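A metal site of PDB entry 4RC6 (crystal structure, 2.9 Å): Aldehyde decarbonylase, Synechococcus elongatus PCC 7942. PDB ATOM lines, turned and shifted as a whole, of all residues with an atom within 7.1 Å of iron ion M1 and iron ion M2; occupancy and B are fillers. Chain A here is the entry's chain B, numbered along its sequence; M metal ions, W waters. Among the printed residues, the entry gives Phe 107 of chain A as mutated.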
ATOM      1  N   VAL A  13      19.521   6.000 -10.406  1.00  0.00           N
ATOM      2  CA  VAL A  13      19.075   6.760 -11.577  1.00  0.00           C
ATOM      3  C   VAL A  13      17.670   7.274 -11.335  1.00  0.00           C
ATOM      4  O   VAL A  13      17.423   8.452 -11.584  1.00  0.00           O
ATOM      5  CB  VAL A  13      19.111   5.952 -12.913  1.00  0.00           C
ATOM      6  CG1 VAL A  13      20.522   5.562 -13.285  1.00  0.00           C
ATOM      7  CG2 VAL A  13      18.167   4.770 -12.898  1.00  0.00           C
ATOM      8  N   GLY A  16      18.130   9.860  -8.779  1.00  0.00           N
ATOM      9  CA  GLY A  16      18.779  10.927  -9.527  1.00  0.00           C
ATOM     10  C   GLY A  16      17.797  11.612 -10.457  1.00  0.00           C
ATOM     11  O   GLY A  16      17.779  12.843 -10.568  1.00  0.00           O
ATOM     12  N   GLU A  17      16.945  10.815 -11.109  1.00  0.00           N
ATOM     13  CA  GLU A  17      16.030  11.405 -12.069  1.00  0.00           C
ATOM     14  C   GLU A  17      14.974  12.198 -11.321  1.00  0.00           C
ATOM     15  O   GLU A  17      14.577  13.233 -11.840  1.00  0.00           O
ATOM     16  CB  GLU A  17      15.359  10.381 -12.991  1.00  0.00           C
ATOM     17  CG  GLU A  17      16.263   9.634 -14.041  1.00  0.00           C
ATOM     18  CD  GLU A  17      16.745  10.486 -15.223  1.00  0.00           C
ATOM     19  OE1 GLU A  17      16.462  11.702 -15.261  1.00  0.00           O
ATOM     20  OE2 GLU A  17      17.448   9.947 -16.120  1.00  0.00           O
ATOM     21  N   ALA A  20      16.482  15.599 -10.102  1.00  0.00           N
ATOM     22  CA  ALA A  20      16.536  16.350 -11.333  1.00  0.00           C
ATOM     23  C   ALA A  20      15.164  16.882 -11.719  1.00  0.00           C
ATOM     24  O   ALA A  20      15.053  18.001 -12.207  1.00  0.00           O
ATOM     25  CB  ALA A  20      17.087  15.472 -12.416  1.00  0.00           C
ATOM     26  N   PHE A  21      14.114  16.083 -11.519  1.00  0.00           N
ATOM     27  CA  PHE A  21      12.726  16.576 -11.680  1.00  0.00           C
ATOM     28  C   PHE A  21      12.370  17.805 -10.827  1.00  0.00           C
ATOM     29  O   PHE A  21      12.078  18.859 -11.387  1.00  0.00           O
ATOM     30  CB  PHE A  21      11.753  15.417 -11.392  1.00  0.00           C
ATOM     31  CG  PHE A  21      10.352  15.841 -10.984  1.00  0.00           C
ATOM     32  CD1 PHE A  21       9.440  16.386 -11.850  1.00  0.00           C
ATOM     33  CD2 PHE A  21       9.955  15.631  -9.670  1.00  0.00           C
ATOM     34  CE1 PHE A  21       8.164  16.737 -11.367  1.00  0.00           C
ATOM     35  CE2 PHE A  21       8.701  15.953  -9.207  1.00  0.00           C
ATOM     36  CZ  PHE A  21       7.811  16.501 -10.056  1.00  0.00           C
ATOM     37  N   TYR A  24      14.802  20.978 -11.288  1.00  0.00           N
ATOM     38  CA  TYR A  24      14.509  21.880 -12.390  1.00  0.00           C
ATOM     39  C   TYR A  24      13.199  22.680 -12.095  1.00  0.00           C
ATOM     40  O   TYR A  24      13.191  23.912 -12.216  1.00  0.00           O
ATOM     41  CB  TYR A  24      14.441  21.111 -13.721  1.00  0.00           C
ATOM     42  CG  TYR A  24      15.799  20.753 -14.311  1.00  0.00           C
ATOM     43  CD1 TYR A  24      16.750  21.728 -14.605  1.00  0.00           C
ATOM     44  CD2 TYR A  24      16.149  19.428 -14.543  1.00  0.00           C
ATOM     45  CE1 TYR A  24      18.020  21.383 -15.148  1.00  0.00           C
ATOM     46  CE2 TYR A  24      17.401  19.082 -15.065  1.00  0.00           C
ATOM     47  CZ  TYR A  24      18.331  20.064 -15.368  1.00  0.00           C
ATOM     48  OH  TYR A  24      19.547  19.695 -15.865  1.00  0.00           O
ATOM     49  N   LEU A  41      12.192  20.726 -19.263  1.00  0.00           N
ATOM     50  CA  LEU A  41      13.331  19.945 -18.731  1.00  0.00           C
ATOM     51  C   LEU A  41      12.897  19.162 -17.497  1.00  0.00           C
ATOM     52  O   LEU A  41      13.163  17.957 -17.398  1.00  0.00           O
ATOM     53  CB  LEU A  41      14.531  20.822 -18.385  1.00  0.00           C
ATOM     54  CG  LEU A  41      15.171  21.686 -19.480  1.00  0.00           C
ATOM     55  CD1 LEU A  41      16.350  22.473 -18.915  1.00  0.00           C
ATOM     56  CD2 LEU A  41      15.561  20.862 -20.714  1.00  0.00           C
ATOM     57  N   MET A  44      10.108  16.372 -18.098  1.00  0.00           N
ATOM     58  CA  MET A  44      10.617  15.473 -19.106  1.00  0.00           C
ATOM     59  C   MET A  44      11.303  14.328 -18.422  1.00  0.00           C
ATOM     60  O   MET A  44      11.046  13.176 -18.697  1.00  0.00           O
ATOM     61  CB  MET A  44      11.695  16.171 -19.894  1.00  0.00           C
ATOM     62  CG  MET A  44      12.542  15.336 -20.783  1.00  0.00           C
ATOM     63  SD  MET A  44      13.464  16.641 -21.589  1.00  0.00           S
ATOM     64  CE  MET A  44      14.246  15.765 -22.902  1.00  0.00           C
ATOM     65  N   GLU A  45      12.121  14.676 -17.437  1.00  0.00           N
ATOM     66  CA  GLU A  45      12.878  13.717 -16.640  1.00  0.00           C
ATOM     67  C   GLU A  45      11.964  12.665 -16.013  1.00  0.00           C
ATOM     68  O   GLU A  45      12.377  11.536 -15.770  1.00  0.00           O
ATOM     69  CB  GLU A  45      13.630  14.465 -15.585  1.00  0.00           C
ATOM     70  CG  GLU A  45      14.651  15.325 -16.259  1.00  0.00           C
ATOM     71  CD  GLU A  45      15.986  15.267 -15.620  1.00  0.00           C
ATOM     72  OE1 GLU A  45      16.291  14.239 -14.984  1.00  0.00           O
ATOM     73  OE2 GLU A  45      16.758  16.229 -15.788  1.00  0.00           O
ATOM     74  N   GLN A  46      10.718  13.042 -15.845  1.00  0.00           N
ATOM     75  CA  GLN A  46       9.649  12.218 -15.331  1.00  0.00           C
ATOM     76  C   GLN A  46       9.478  10.932 -16.156  1.00  0.00           C
ATOM     77  O   GLN A  46       9.203   9.853 -15.650  1.00  0.00           O
ATOM     78  CB  GLN A  46       8.411  13.074 -15.417  1.00  0.00           C
ATOM     79  CG  GLN A  46       7.281  12.680 -14.514  1.00  0.00           C
ATOM     80  CD  GLN A  46       6.029  12.316 -15.282  1.00  0.00           C
ATOM     81  OE1 GLN A  46       5.950  12.429 -16.490  1.00  0.00           O
ATOM     82  NE2 GLN A  46       5.032  11.845 -14.566  1.00  0.00           N
ATOM     83  N   HIS A  48      11.879   9.723 -17.942  1.00  0.00           N
ATOM     84  CA  HIS A  48      13.140   9.005 -17.776  1.00  0.00           C
ATOM     85  C   HIS A  48      12.991   8.145 -16.500  1.00  0.00           C
ATOM     86  O   HIS A  48      13.298   6.950 -16.496  1.00  0.00           O
ATOM     87  CB  HIS A  48      14.354   9.952 -17.657  1.00  0.00           C
ATOM     88  CG  HIS A  48      14.494  10.952 -18.761  1.00  0.00           C
ATOM     89  ND1 HIS A  48      15.707  11.433 -19.194  1.00  0.00           N
ATOM     90  CD2 HIS A  48      13.562  11.624 -19.473  1.00  0.00           C
ATOM     91  CE1 HIS A  48      15.529  12.305 -20.162  1.00  0.00           C
ATOM     92  NE2 HIS A  48      14.227  12.443 -20.346  1.00  0.00           N
ATOM     93  N   MET A  49      12.501   8.797 -15.447  1.00  0.00           N
ATOM     94  CA  MET A  49      12.197   8.173 -14.154  1.00  0.00           C
ATOM     95  C   MET A  49      11.374   6.913 -14.335  1.00  0.00           C
ATOM     96  O   MET A  49      11.742   5.799 -13.899  1.00  0.00           O
ATOM     97  CB  MET A  49      11.424   9.156 -13.281  1.00  0.00           C
ATOM     98  CG  MET A  49      11.042   8.690 -11.892  1.00  0.00           C
ATOM     99  SD  MET A  49      10.705  10.115 -10.813  1.00  0.00           S
ATOM    100  CE  MET A  49      10.198   9.311  -9.290  1.00  0.00           C
ATOM    101  N   PHE A  52      13.187   3.892 -16.364  1.00  0.00           N
ATOM    102  CA  PHE A  52      14.145   2.985 -15.738  1.00  0.00           C
ATOM    103  C   PHE A  52      13.529   1.997 -14.747  1.00  0.00           C
ATOM    104  O   PHE A  52      14.118   0.949 -14.474  1.00  0.00           O
ATOM    105  CB  PHE A  52      15.249   3.811 -15.059  1.00  0.00           C
ATOM    106  CG  PHE A  52      16.157   4.540 -16.026  1.00  0.00           C
ATOM    107  CD1 PHE A  52      16.959   3.821 -16.929  1.00  0.00           C
ATOM    108  CD2 PHE A  52      16.212   5.927 -16.033  1.00  0.00           C
ATOM    109  CE1 PHE A  52      17.779   4.485 -17.825  1.00  0.00           C
ATOM    110  CE2 PHE A  52      17.043   6.592 -16.919  1.00  0.00           C
ATOM    111  CZ  PHE A  52      17.827   5.871 -17.810  1.00  0.00           C
ATOM    112  N   GLN A  95      23.203  21.028 -10.743  1.00  0.00           N
ATOM    113  CA  GLN A  95      22.349  20.190 -11.582  1.00  0.00           C
ATOM    114  C   GLN A  95      22.756  20.102 -13.007  1.00  0.00           C
ATOM    115  O   GLN A  95      23.017  19.071 -13.563  1.00  0.00           O
ATOM    116  CB  GLN A  95      20.924  20.699 -11.570  1.00  0.00           C
ATOM    117  CG  GLN A  95      19.870  19.664 -11.244  1.00  0.00           C
ATOM    118  CD  GLN A  95      19.993  18.392 -12.044  1.00  0.00           C
ATOM    119  OE1 GLN A  95      21.048  17.954 -12.393  1.00  0.00           O
ATOM    120  NE2 GLN A  95      18.877  17.810 -12.336  1.00  0.00           N
ATOM    121  N   ILE A  99      25.647  16.932 -12.168  1.00  0.00           N
ATOM    122  CA  ILE A  99      24.776  15.755 -12.220  1.00  0.00           C
ATOM    123  C   ILE A  99      24.538  15.273 -13.656  1.00  0.00           C
ATOM    124  O   ILE A  99      24.638  14.089 -13.928  1.00  0.00           O
ATOM    125  CB  ILE A  99      23.401  15.997 -11.510  1.00  0.00           C
ATOM    126  CG1 ILE A  99      23.574  16.124  -9.984  1.00  0.00           C
ATOM    127  CG2 ILE A  99      22.427  14.846 -11.786  1.00  0.00           C
ATOM    128  CD1 ILE A  99      22.258  16.167  -9.175  1.00  0.00           C
ATOM    129  N   GLU A 100      24.221  16.163 -14.575  1.00  0.00           N
ATOM    130  CA  GLU A 100      23.975  15.714 -15.942  1.00  0.00           C
ATOM    131  C   GLU A 100      25.244  15.112 -16.579  1.00  0.00           C
ATOM    132  O   GLU A 100      25.143  14.102 -17.308  1.00  0.00           O
ATOM    133  CB  GLU A 100      23.387  16.851 -16.784  1.00  0.00           C
ATOM    134  CG  GLU A 100      22.142  17.526 -16.144  1.00  0.00           C
ATOM    135  CD  GLU A 100      20.842  16.659 -16.121  1.00  0.00           C
ATOM    136  OE1 GLU A 100      20.904  15.415 -16.325  1.00  0.00           O
ATOM    137  OE2 GLU A 100      19.733  17.236 -15.877  1.00  0.00           O
ATOM    138  N   ALA A 103      25.242  11.775 -15.201  1.00  0.00           N
ATOM    139  CA  ALA A 103      24.305  10.934 -15.943  1.00  0.00           C
ATOM    140  C   ALA A 103      24.864  10.524 -17.299  1.00  0.00           C
ATOM    141  O   ALA A 103      24.865   9.335 -17.662  1.00  0.00           O
ATOM    142  CB  ALA A 103      22.984  11.645 -16.113  1.00  0.00           C
ATOM    143  N   PHE A 107      25.430   6.401 -18.408  1.00  0.00           N
ATOM    144  CA  PHE A 107      24.667   5.821 -19.504  1.00  0.00           C
ATOM    145  C   PHE A 107      25.568   5.390 -20.665  1.00  0.00           C
ATOM    146  O   PHE A 107      25.424   4.274 -21.212  1.00  0.00           O
ATOM    147  CB  PHE A 107      23.609   6.804 -20.015  1.00  0.00           C
ATOM    148  CG  PHE A 107      22.709   7.362 -18.923  1.00  0.00           C
ATOM    149  CD1 PHE A 107      22.555   6.701 -17.690  1.00  0.00           C
ATOM    150  CD2 PHE A 107      21.961   8.526 -19.150  1.00  0.00           C
ATOM    151  CE1 PHE A 107      21.719   7.230 -16.701  1.00  0.00           C
ATOM    152  CE2 PHE A 107      21.113   9.063 -18.181  1.00  0.00           C
ATOM    153  CZ  PHE A 107      20.985   8.424 -16.962  1.00  0.00           C
ATOM    154  N   VAL A 125      16.870   8.247 -23.381  1.00  0.00           N
ATOM    155  CA  VAL A 125      17.227   9.203 -22.327  1.00  0.00           C
ATOM    156  C   VAL A 125      18.515  10.007 -22.556  1.00  0.00           C
ATOM    157  O   VAL A 125      18.554  11.216 -22.288  1.00  0.00           O
ATOM    158  CB  VAL A 125      17.322   8.486 -20.970  1.00  0.00           C
ATOM    159  CG1 VAL A 125      18.061   9.331 -19.950  1.00  0.00           C
ATOM    160  CG2 VAL A 125      15.931   8.141 -20.451  1.00  0.00           C
ATOM    161  N   ASP A 128      18.999  13.356 -24.287  1.00  0.00           N
ATOM    162  CA  ASP A 128      18.304  14.419 -23.587  1.00  0.00           C
ATOM    163  C   ASP A 128      19.121  15.076 -22.481  1.00  0.00           C
ATOM    164  O   ASP A 128      18.901  16.232 -22.108  1.00  0.00           O
ATOM    165  CB  ASP A 128      17.012  13.835 -23.020  1.00  0.00           C
ATOM    166  CG  ASP A 128      15.999  13.519 -24.123  1.00  0.00           C
ATOM    167  OD1 ASP A 128      16.224  13.951 -25.276  1.00  0.00           O
ATOM    168  OD2 ASP A 128      14.983  12.849 -23.854  1.00  0.00           O
ATOM    169  N   GLU A 129      20.047  14.313 -21.933  1.00  0.00           N
ATOM    170  CA  GLU A 129      20.878  14.809 -20.847  1.00  0.00           C
ATOM    171  C   GLU A 129      21.885  15.891 -21.304  1.00  0.00           C
ATOM    172  O   GLU A 129      22.154  16.840 -20.564  1.00  0.00           O
ATOM    173  CB  GLU A 129      21.576  13.602 -20.221  1.00  0.00           C
ATOM    174  CG  GLU A 129      20.584  12.485 -19.864  1.00  0.00           C
ATOM    175  CD  GLU A 129      19.587  12.833 -18.740  1.00  0.00           C
ATOM    176  OE1 GLU A 129      19.548  13.995 -18.261  1.00  0.00           O
ATOM    177  OE2 GLU A 129      18.786  11.941 -18.363  1.00  0.00           O
ATOM    178  N   HIS A 132      20.123  19.142 -21.164  1.00  0.00           N
ATOM    179  CA  HIS A 132      20.069  19.658 -19.797  1.00  0.00           C
ATOM    180  C   HIS A 132      21.383  20.395 -19.481  1.00  0.00           C
ATOM    181  O   HIS A 132      21.353  21.510 -18.949  1.00  0.00           O
ATOM    182  CB  HIS A 132      19.791  18.525 -18.814  1.00  0.00           C
ATOM    183  CG  HIS A 132      18.437  17.913 -18.984  1.00  0.00           C
ATOM    184  ND1 HIS A 132      18.134  16.634 -18.562  1.00  0.00           N
ATOM    185  CD2 HIS A 132      17.289  18.411 -19.506  1.00  0.00           C
ATOM    186  CE1 HIS A 132      16.866  16.367 -18.843  1.00  0.00           C
ATOM    187  NE2 HIS A 132      16.329  17.434 -19.413  1.00  0.00           N
ATOM    188  N   ARG A 133      22.511  19.802 -19.865  1.00  0.00           N
ATOM    189  CA  ARG A 133      23.815  20.455 -19.754  1.00  0.00           C
ATOM    190  C   ARG A 133      23.799  21.801 -20.506  1.00  0.00           C
ATOM    191  O   ARG A 133      24.402  22.780 -20.058  1.00  0.00           O
ATOM    192  CB  ARG A 133      24.947  19.533 -20.258  1.00  0.00           C
ATOM    193  CG  ARG A 133      26.234  20.296 -20.666  1.00  0.00           C
ATOM    194  CD  ARG A 133      27.532  19.594 -20.293  1.00  0.00           C
ATOM    195  NE  ARG A 133      27.939  18.508 -21.199  1.00  0.00           N
ATOM    196  CZ  ARG A 133      28.772  18.641 -22.232  1.00  0.00           C
ATOM    197  NH1 ARG A 133      29.309  19.812 -22.525  1.00  0.00           N
ATOM    198  NH2 ARG A 133      29.079  17.585 -22.971  1.00  0.00           N
HETATM  199 FE    FE M   1      17.340  12.826 -16.665  1.00  0.00          FE
HETATM  200 FE    FE M   2      18.570  15.279 -16.507  1.00  0.00          FE
HETATM  201  O   HOH W   1      19.615  13.639 -14.070  1.00  0.00           O
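OE2 of Glu 100 sits close to OH of Tyr 24 (2.5 Å). The backbone carbonyl oxygen of Gln 95 sits close to the backbone NH of Glu 100 (3.3 Å). The side-chain carboxylate of Glu 129 sits close to a ring nitrogen (ND1) of His 48, 3.2 Å away. A ring nitrogen (NE2) of His 132 sits at hydrogen-bond distance from the side-chain sulfur (SD) of Met 44, at 3.7 Å.
ND1 of His 48 touches iron ion M1 (3.3 Å). Of the 23 residues printed, 4 come within 4 Å of iron ion M1.
Within 4 Å of iron ion M2: Glu 45, Glu 100, Glu 129 and His 132.
Iron ion M1 is bound by the side-chain carboxylate (OE1) of Glu 17, 2.0 Å away. Iron ion M1 is bound by OE2 of Glu 129 (2.4 Å). Iron ion M1 is bound by OE1 of Glu 45 (2.4 Å).
OE2 of Glu 45 is bound to iron ion M2 (2.2 Å). OE1 of Glu 100 is bound to iron ion M2, at 2.3 Å. Iron ion M2 is bound by the side-chain carboxylate (OE2) of Glu 100, at 2.4 Å. Iron ion M2 is bound by the side-chain carboxylate (OE1) of Glu 129 (2.4 Å). A ring nitrogen (ND1) of His 132 is bound to iron ion M2.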
